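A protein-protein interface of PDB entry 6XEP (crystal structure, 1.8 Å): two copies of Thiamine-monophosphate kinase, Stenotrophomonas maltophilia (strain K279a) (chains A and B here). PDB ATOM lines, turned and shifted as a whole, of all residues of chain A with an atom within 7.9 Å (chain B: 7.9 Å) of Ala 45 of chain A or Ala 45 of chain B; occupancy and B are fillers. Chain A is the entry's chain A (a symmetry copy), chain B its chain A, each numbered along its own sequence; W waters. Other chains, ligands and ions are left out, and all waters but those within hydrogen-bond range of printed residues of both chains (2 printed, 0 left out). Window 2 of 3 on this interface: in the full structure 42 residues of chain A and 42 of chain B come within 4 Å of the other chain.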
ATOM      1  N   LEU A  41     -20.705 -17.978 -25.970  1.00  0.00           N
ATOM      2  CA  LEU A  41     -21.696 -16.986 -26.361  1.00  0.00           C
ATOM      3  C   LEU A  41     -21.028 -15.669 -26.737  1.00  0.00           C
ATOM      4  O   LEU A  41     -20.054 -15.243 -26.097  1.00  0.00           O
ATOM      5  CB  LEU A  41     -22.690 -16.741 -25.234  1.00  0.00           C
ATOM      6  CG  LEU A  41     -23.143 -18.023 -24.528  1.00  0.00           C
ATOM      7  CD1 LEU A  41     -23.900 -17.682 -23.258  1.00  0.00           C
ATOM      8  CD2 LEU A  41     -23.987 -18.862 -25.467  1.00  0.00           C
ATOM      9  N   GLN A  42     -21.556 -15.023 -27.782  1.00  0.00           N
ATOM     10  CA  GLN A  42     -21.027 -13.743 -28.242  1.00  0.00           C
ATOM     11  C   GLN A  42     -22.033 -12.631 -27.957  1.00  0.00           C
ATOM     12  O   GLN A  42     -23.031 -12.497 -28.686  1.00  0.00           O
ATOM     13  CB  GLN A  42     -20.699 -13.792 -29.735  1.00  0.00           C
ATOM     14  CG  GLN A  42     -20.025 -12.522 -30.241  1.00  0.00           C
ATOM     15  CD  GLN A  42     -18.748 -12.205 -29.489  1.00  0.00           C
ATOM     16  OE1 GLN A  42     -17.751 -12.915 -29.614  1.00  0.00           O
ATOM     17  NE2 GLN A  42     -18.772 -11.136 -28.698  1.00  0.00           N
ATOM     18  N   PRO A  43     -21.832 -11.821 -26.921  1.00  0.00           N
ATOM     19  CA  PRO A  43     -22.754 -10.710 -26.666  1.00  0.00           C
ATOM     20  C   PRO A  43     -22.617  -9.658 -27.751  1.00  0.00           C
ATOM     21  O   PRO A  43     -21.623  -9.609 -28.479  1.00  0.00           O
ATOM     22  CB  PRO A  43     -22.298 -10.159 -25.307  1.00  0.00           C
ATOM     23  CG  PRO A  43     -21.363 -11.220 -24.740  1.00  0.00           C
ATOM     24  CD  PRO A  43     -20.748 -11.878 -25.928  1.00  0.00           C
ATOM     25  N   ARG A  44     -23.626  -8.799 -27.860  1.00  0.00           N
ATOM     26  CA  ARG A  44     -23.447  -7.616 -28.699  1.00  0.00           C
ATOM     27  C   ARG A  44     -22.604  -6.585 -27.955  1.00  0.00           C
ATOM     28  O   ARG A  44     -22.883  -6.249 -26.797  1.00  0.00           O
ATOM     29  CB  ARG A  44     -24.786  -7.026 -29.126  1.00  0.00           C
ATOM     30  CG  ARG A  44     -25.642  -8.004 -29.945  1.00  0.00           C
ATOM     31  CD  ARG A  44     -26.898  -7.310 -30.453  1.00  0.00           C
ATOM     32  NE  ARG A  44     -27.742  -8.163 -31.283  1.00  0.00           N
ATOM     33  CZ  ARG A  44     -28.886  -7.764 -31.837  1.00  0.00           C
ATOM     34  NH1 ARG A  44     -29.595  -8.606 -32.579  1.00  0.00           N
ATOM     35  NH2 ARG A  44     -29.328  -6.524 -31.649  1.00  0.00           N
ATOM     36  N   ALA A  45     -21.567  -6.090 -28.635  1.00  0.00           N
ATOM     37  CA  ALA A  45     -20.567  -5.248 -27.988  1.00  0.00           C
ATOM     38  C   ALA A  45     -21.165  -3.952 -27.450  1.00  0.00           C
ATOM     39  O   ALA A  45     -20.802  -3.506 -26.353  1.00  0.00           O
ATOM     40  CB  ALA A  45     -19.443  -4.940 -28.970  1.00  0.00           C
ATOM     41  N   ASN A  46     -22.056  -3.315 -28.207  1.00  0.00           N
ATOM     42  CA  ASN A  46     -22.614  -2.045 -27.752  1.00  0.00           C
ATOM     43  C   ASN A  46     -23.878  -2.214 -26.921  1.00  0.00           C
ATOM     44  O   ASN A  46     -24.473  -1.207 -26.529  1.00  0.00           O
ATOM     45  CB  ASN A  46     -22.908  -1.119 -28.942  1.00  0.00           C
ATOM     46  N   GLU A  47     -24.291  -3.441 -26.622  1.00  0.00           N
ATOM     47  CA  GLU A  47     -25.477  -3.660 -25.813  1.00  0.00           C
ATOM     48  C   GLU A  47     -25.077  -4.125 -24.419  1.00  0.00           C
ATOM     49  O   GLU A  47     -23.954  -4.578 -24.183  1.00  0.00           O
ATOM     50  CB  GLU A  47     -26.423  -4.671 -26.478  1.00  0.00           C
ATOM     51  CG  GLU A  47     -26.982  -4.117 -27.783  1.00  0.00           C
ATOM     52  CD  GLU A  47     -28.212  -4.840 -28.291  1.00  0.00           C
ATOM     53  OE1 GLU A  47     -28.715  -5.741 -27.592  1.00  0.00           O
ATOM     54  OE2 GLU A  47     -28.676  -4.508 -29.407  1.00  0.00           O
ATOM     55  N   GLN A  48     -26.000  -3.966 -23.485  1.00  0.00           N
ATOM     56  CA  GLN A  48     -25.795  -4.441 -22.128  1.00  0.00           C
ATOM     57  C   GLN A  48     -26.631  -5.687 -21.883  1.00  0.00           C
ATOM     58  O   GLN A  48     -27.692  -5.876 -22.486  1.00  0.00           O
ATOM     59  CB  GLN A  48     -26.132  -3.349 -21.116  1.00  0.00           C
ATOM     60  CG  GLN A  48     -25.120  -2.214 -21.145  1.00  0.00           C
ATOM     61  CD  GLN A  48     -25.620  -0.974 -20.462  1.00  0.00           C
ATOM     62  OE1 GLN A  48     -26.683  -0.452 -20.800  1.00  0.00           O
ATOM     63  NE2 GLN A  48     -24.869  -0.501 -19.475  1.00  0.00           N
ATOM     64  N   GLN A 144     -30.717  -8.690 -23.731  1.00  0.00           N
ATOM     65  CA  GLN A 144     -29.827  -7.592 -24.071  1.00  0.00           C
ATOM     66  C   GLN A 144     -30.631  -6.327 -24.321  1.00  0.00           C
ATOM     67  O   GLN A 144     -31.765  -6.390 -24.801  1.00  0.00           O
ATOM     68  CB  GLN A 144     -28.971  -7.955 -25.288  1.00  0.00           C
ATOM     69  CG  GLN A 144     -28.108  -9.169 -24.991  1.00  0.00           C
ATOM     70  CD  GLN A 144     -27.168  -9.526 -26.108  1.00  0.00           C
ATOM     71  OE1 GLN A 144     -25.995  -9.131 -26.101  1.00  0.00           O
ATOM     72  NE2 GLN A 144     -27.664 -10.300 -27.069  1.00  0.00           N
ATOM     73  N   LEU B  41     -25.141  -5.345 -17.151  1.00  0.00           N
ATOM     74  CA  LEU B  41     -23.789  -5.880 -17.234  1.00  0.00           C
ATOM     75  C   LEU B  41     -23.150  -5.539 -18.575  1.00  0.00           C
ATOM     76  O   LEU B  41     -23.814  -5.572 -19.623  1.00  0.00           O
ATOM     77  CB  LEU B  41     -23.794  -7.391 -17.049  1.00  0.00           C
ATOM     78  CG  LEU B  41     -24.727  -7.869 -15.932  1.00  0.00           C
ATOM     79  CD1 LEU B  41     -24.890  -9.375 -15.994  1.00  0.00           C
ATOM     80  CD2 LEU B  41     -24.195  -7.424 -14.585  1.00  0.00           C
ATOM     81  N   GLN B  42     -21.855  -5.211 -18.539  1.00  0.00           N
ATOM     82  CA  GLN B  42     -21.113  -4.879 -19.750  1.00  0.00           C
ATOM     83  C   GLN B  42     -20.093  -5.972 -20.054  1.00  0.00           C
ATOM     84  O   GLN B  42     -19.034  -6.031 -19.404  1.00  0.00           O
ATOM     85  CB  GLN B  42     -20.413  -3.526 -19.608  1.00  0.00           C
ATOM     86  CG  GLN B  42     -19.726  -3.070 -20.890  1.00  0.00           C
ATOM     87  CD  GLN B  42     -20.685  -2.982 -22.061  1.00  0.00           C
ATOM     88  OE1 GLN B  42     -21.561  -2.120 -22.094  1.00  0.00           O
ATOM     89  NE2 GLN B  42     -20.526  -3.880 -23.029  1.00  0.00           N
ATOM     90  N   PRO B  43     -20.355  -6.860 -21.009  1.00  0.00           N
ATOM     91  CA  PRO B  43     -19.363  -7.883 -21.357  1.00  0.00           C
ATOM     92  C   PRO B  43     -18.164  -7.239 -22.027  1.00  0.00           C
ATOM     93  O   PRO B  43     -18.229  -6.111 -22.520  1.00  0.00           O
ATOM     94  CB  PRO B  43     -20.110  -8.803 -22.333  1.00  0.00           C
ATOM     95  CG  PRO B  43     -21.578  -8.418 -22.199  1.00  0.00           C
ATOM     96  CD  PRO B  43     -21.574  -6.975 -21.825  1.00  0.00           C
ATOM     97  N   ARG B  44     -17.051  -7.967 -22.055  1.00  0.00           N
ATOM     98  CA  ARG B  44     -15.947  -7.522 -22.902  1.00  0.00           C
ATOM     99  C   ARG B  44     -16.249  -7.867 -24.356  1.00  0.00           C
ATOM    100  O   ARG B  44     -16.604  -9.007 -24.681  1.00  0.00           O
ATOM    101  CB  ARG B  44     -14.621  -8.130 -22.457  1.00  0.00           C
ATOM    102  CG  ARG B  44     -14.236  -7.748 -21.019  1.00  0.00           C
ATOM    103  CD  ARG B  44     -12.845  -8.272 -20.688  1.00  0.00           C
ATOM    104  NE  ARG B  44     -12.387  -7.907 -19.352  1.00  0.00           N
ATOM    105  CZ  ARG B  44     -11.201  -8.254 -18.853  1.00  0.00           C
ATOM    106  NH1 ARG B  44     -10.862  -7.881 -17.625  1.00  0.00           N
ATOM    107  NH2 ARG B  44     -10.351  -8.976 -19.577  1.00  0.00           N
ATOM    108  N   ALA B  45     -16.106  -6.865 -25.227  1.00  0.00           N
ATOM    109  CA  ALA B  45     -16.544  -6.995 -26.613  1.00  0.00           C
ATOM    110  C   ALA B  45     -15.790  -8.093 -27.356  1.00  0.00           C
ATOM    111  O   ALA B  45     -16.389  -8.839 -28.142  1.00  0.00           O
ATOM    112  CB  ALA B  45     -16.374  -5.661 -27.331  1.00  0.00           C
ATOM    113  N   ASN B  46     -14.478  -8.196 -27.151  1.00  0.00           N
ATOM    114  CA  ASN B  46     -13.710  -9.199 -27.882  1.00  0.00           C
ATOM    115  C   ASN B  46     -13.631 -10.534 -27.156  1.00  0.00           C
ATOM    116  O   ASN B  46     -12.959 -11.444 -27.649  1.00  0.00           O
ATOM    117  CB  ASN B  46     -12.288  -8.695 -28.174  1.00  0.00           C
ATOM    118  N   GLU B  47     -14.308 -10.690 -26.023  1.00  0.00           N
ATOM    119  CA  GLU B  47     -14.288 -11.949 -25.299  1.00  0.00           C
ATOM    120  C   GLU B  47     -15.620 -12.667 -25.469  1.00  0.00           C
ATOM    121  O   GLU B  47     -16.634 -12.075 -25.849  1.00  0.00           O
ATOM    122  CB  GLU B  47     -13.967 -11.730 -23.813  1.00  0.00           C
ATOM    123  CG  GLU B  47     -12.550 -11.197 -23.636  1.00  0.00           C
ATOM    124  CD  GLU B  47     -12.002 -11.340 -22.230  1.00  0.00           C
ATOM    125  OE1 GLU B  47     -12.683 -11.939 -21.375  1.00  0.00           O
ATOM    126  OE2 GLU B  47     -10.882 -10.839 -21.978  1.00  0.00           O
ATOM    127  N   GLN B  48     -15.596 -13.966 -25.221  1.00  0.00           N
ATOM    128  CA  GLN B  48     -16.807 -14.767 -25.256  1.00  0.00           C
ATOM    129  C   GLN B  48     -17.234 -15.124 -23.841  1.00  0.00           C
ATOM    130  O   GLN B  48     -16.408 -15.232 -22.930  1.00  0.00           O
ATOM    131  CB  GLN B  48     -16.600 -16.024 -26.097  1.00  0.00           C
ATOM    132  CG  GLN B  48     -16.463 -15.702 -27.578  1.00  0.00           C
ATOM    133  CD  GLN B  48     -15.883 -16.840 -28.367  1.00  0.00           C
ATOM    134  OE1 GLN B  48     -14.799 -17.337 -28.055  1.00  0.00           O
ATOM    135  NE2 GLN B  48     -16.609 -17.281 -29.387  1.00  0.00           N
ATOM    136  N   GLN B 144     -15.670 -15.319 -18.679  1.00  0.00           N
ATOM    137  CA  GLN B 144     -15.300 -14.820 -19.994  1.00  0.00           C
ATOM    138  C   GLN B 144     -13.976 -15.424 -20.428  1.00  0.00           C
ATOM    139  O   GLN B 144     -13.110 -15.702 -19.595  1.00  0.00           O
ATOM    140  CB  GLN B 144     -15.236 -13.290 -19.986  1.00  0.00           C
ATOM    141  CG  GLN B 144     -16.592 -12.700 -19.637  1.00  0.00           C
ATOM    142  CD  GLN B 144     -16.630 -11.199 -19.704  1.00  0.00           C
ATOM    143  OE1 GLN B 144     -17.035 -10.620 -20.721  1.00  0.00           O
ATOM    144  NE2 GLN B 144     -16.233 -10.551 -18.613  1.00  0.00           N
HETATM  145  O   HOH W   1     -22.964  -2.119 -17.550  1.00  0.00           O
HETATM  146  O   HOH W   2     -19.749 -17.230 -29.688  1.00  0.00           O
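Of chain B, only Gln 42 and Ala 45 come within 4 Å of Ala 45 of chain A. Of chain A, only Gln 42 (3.4 Å) and Ala 45 (3.6 Å) come within 4 Å of Ala 45 of chain B. Printed residues of chain B within 4 Å of Glu 47 of chain A: Gln 42. Of the printed residues of chain A, Pro 43 of chain B touches Pro 43. The nearest residue of chain B that does not touch Ala 45 of chain A is Pro 43 of chain B (5.3 Å). The nearest printed residue of chain B that does not touch Glu 47 of chain A is Pro 43 of chain B (4.1 Å).
Gln 48 of chain B touches Leu 41 of chain A. Gln 42 of chain A touches Glu 47 of chain B. CG of Gln 48 of chain B touches OE1 of Gln 42 of chain A, 3.7 Å away. CG of Pro 43 of chain A touches CB of Pro 43 of chain B, at 3.6 Å. Ala 45 of chain A touches Ala 45 of chain B. Glu 47 of chain A touches Gln 42 of chain B. Leu 41 of chain B touches Gln 48 of chain A. Gln 48 of chain A touches Gln 42 of chain B.
Of the 9 printed residues of chain A, 6 touch a printed residue of chain B. Printed residues of chain A that touch a printed residue of chain B: Leu 41, Gln 42, Pro 43, Ala 45, Glu 47 and Gln 48. Of the 9 printed residues of chain B, 6 touch a printed residue of chain A. Hydrophobic or aromatic side chains of chain B within 4 Å of the printed part of chain A: Pro 43 and Ala 45.
The side-chain carboxylate (OE2) of Glu 47 of chain B is in salt-bridge range of the guanidinium group (NH2) of Arg 44 of chain B, at 3.1 Å. The side-chain carboxylate (OE2) of Glu 47 of chain A is in salt-bridge range of the guanidinium group (NH2) of Arg 44 of chain A (3.1 Å).
Leu 41 of chain A touches Gln 48 of chain B, and with the chains exchanged Gln 48 of chain A touches Leu 41 of chain B. Gln 42 of chain A touches Glu 47 of chain B, and with the chains exchanged Glu 47 of chain A touches Gln 42 of chain B. Gln 42 of chain A touches Gln 48 of chain B, and with the chains exchanged Gln 48 of chain A touches Gln 42 of chain B. Pro 43 of chain A touches its own counterpart, Pro 43 of chain B. Of the 10 pairs that touch across the chains among the printed residues, 10 have their exchanged pair printed and touching as well.
NE2 of Gln 42 of chain A sits at hydrogen-bond distance from O of Ala 45 of chain B (3.4 Å). The backbone carbonyl oxygen (O) of Ala 45 of chain A is in hydrogen-bond range of the side-chain amide nitrogen (NE2) of Gln 42 of chain B, at 3.4 Å.
Water W2 bridges the side-chain amide nitrogen of Gln 48 of chain B (3.2 Å) and the backbone NH of Gln 42 of chain A (3.4 Å). Water W1 lies within hydrogen-bond range of NE2 of Gln 48 of chain A and N of Gln 42 of chain B.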
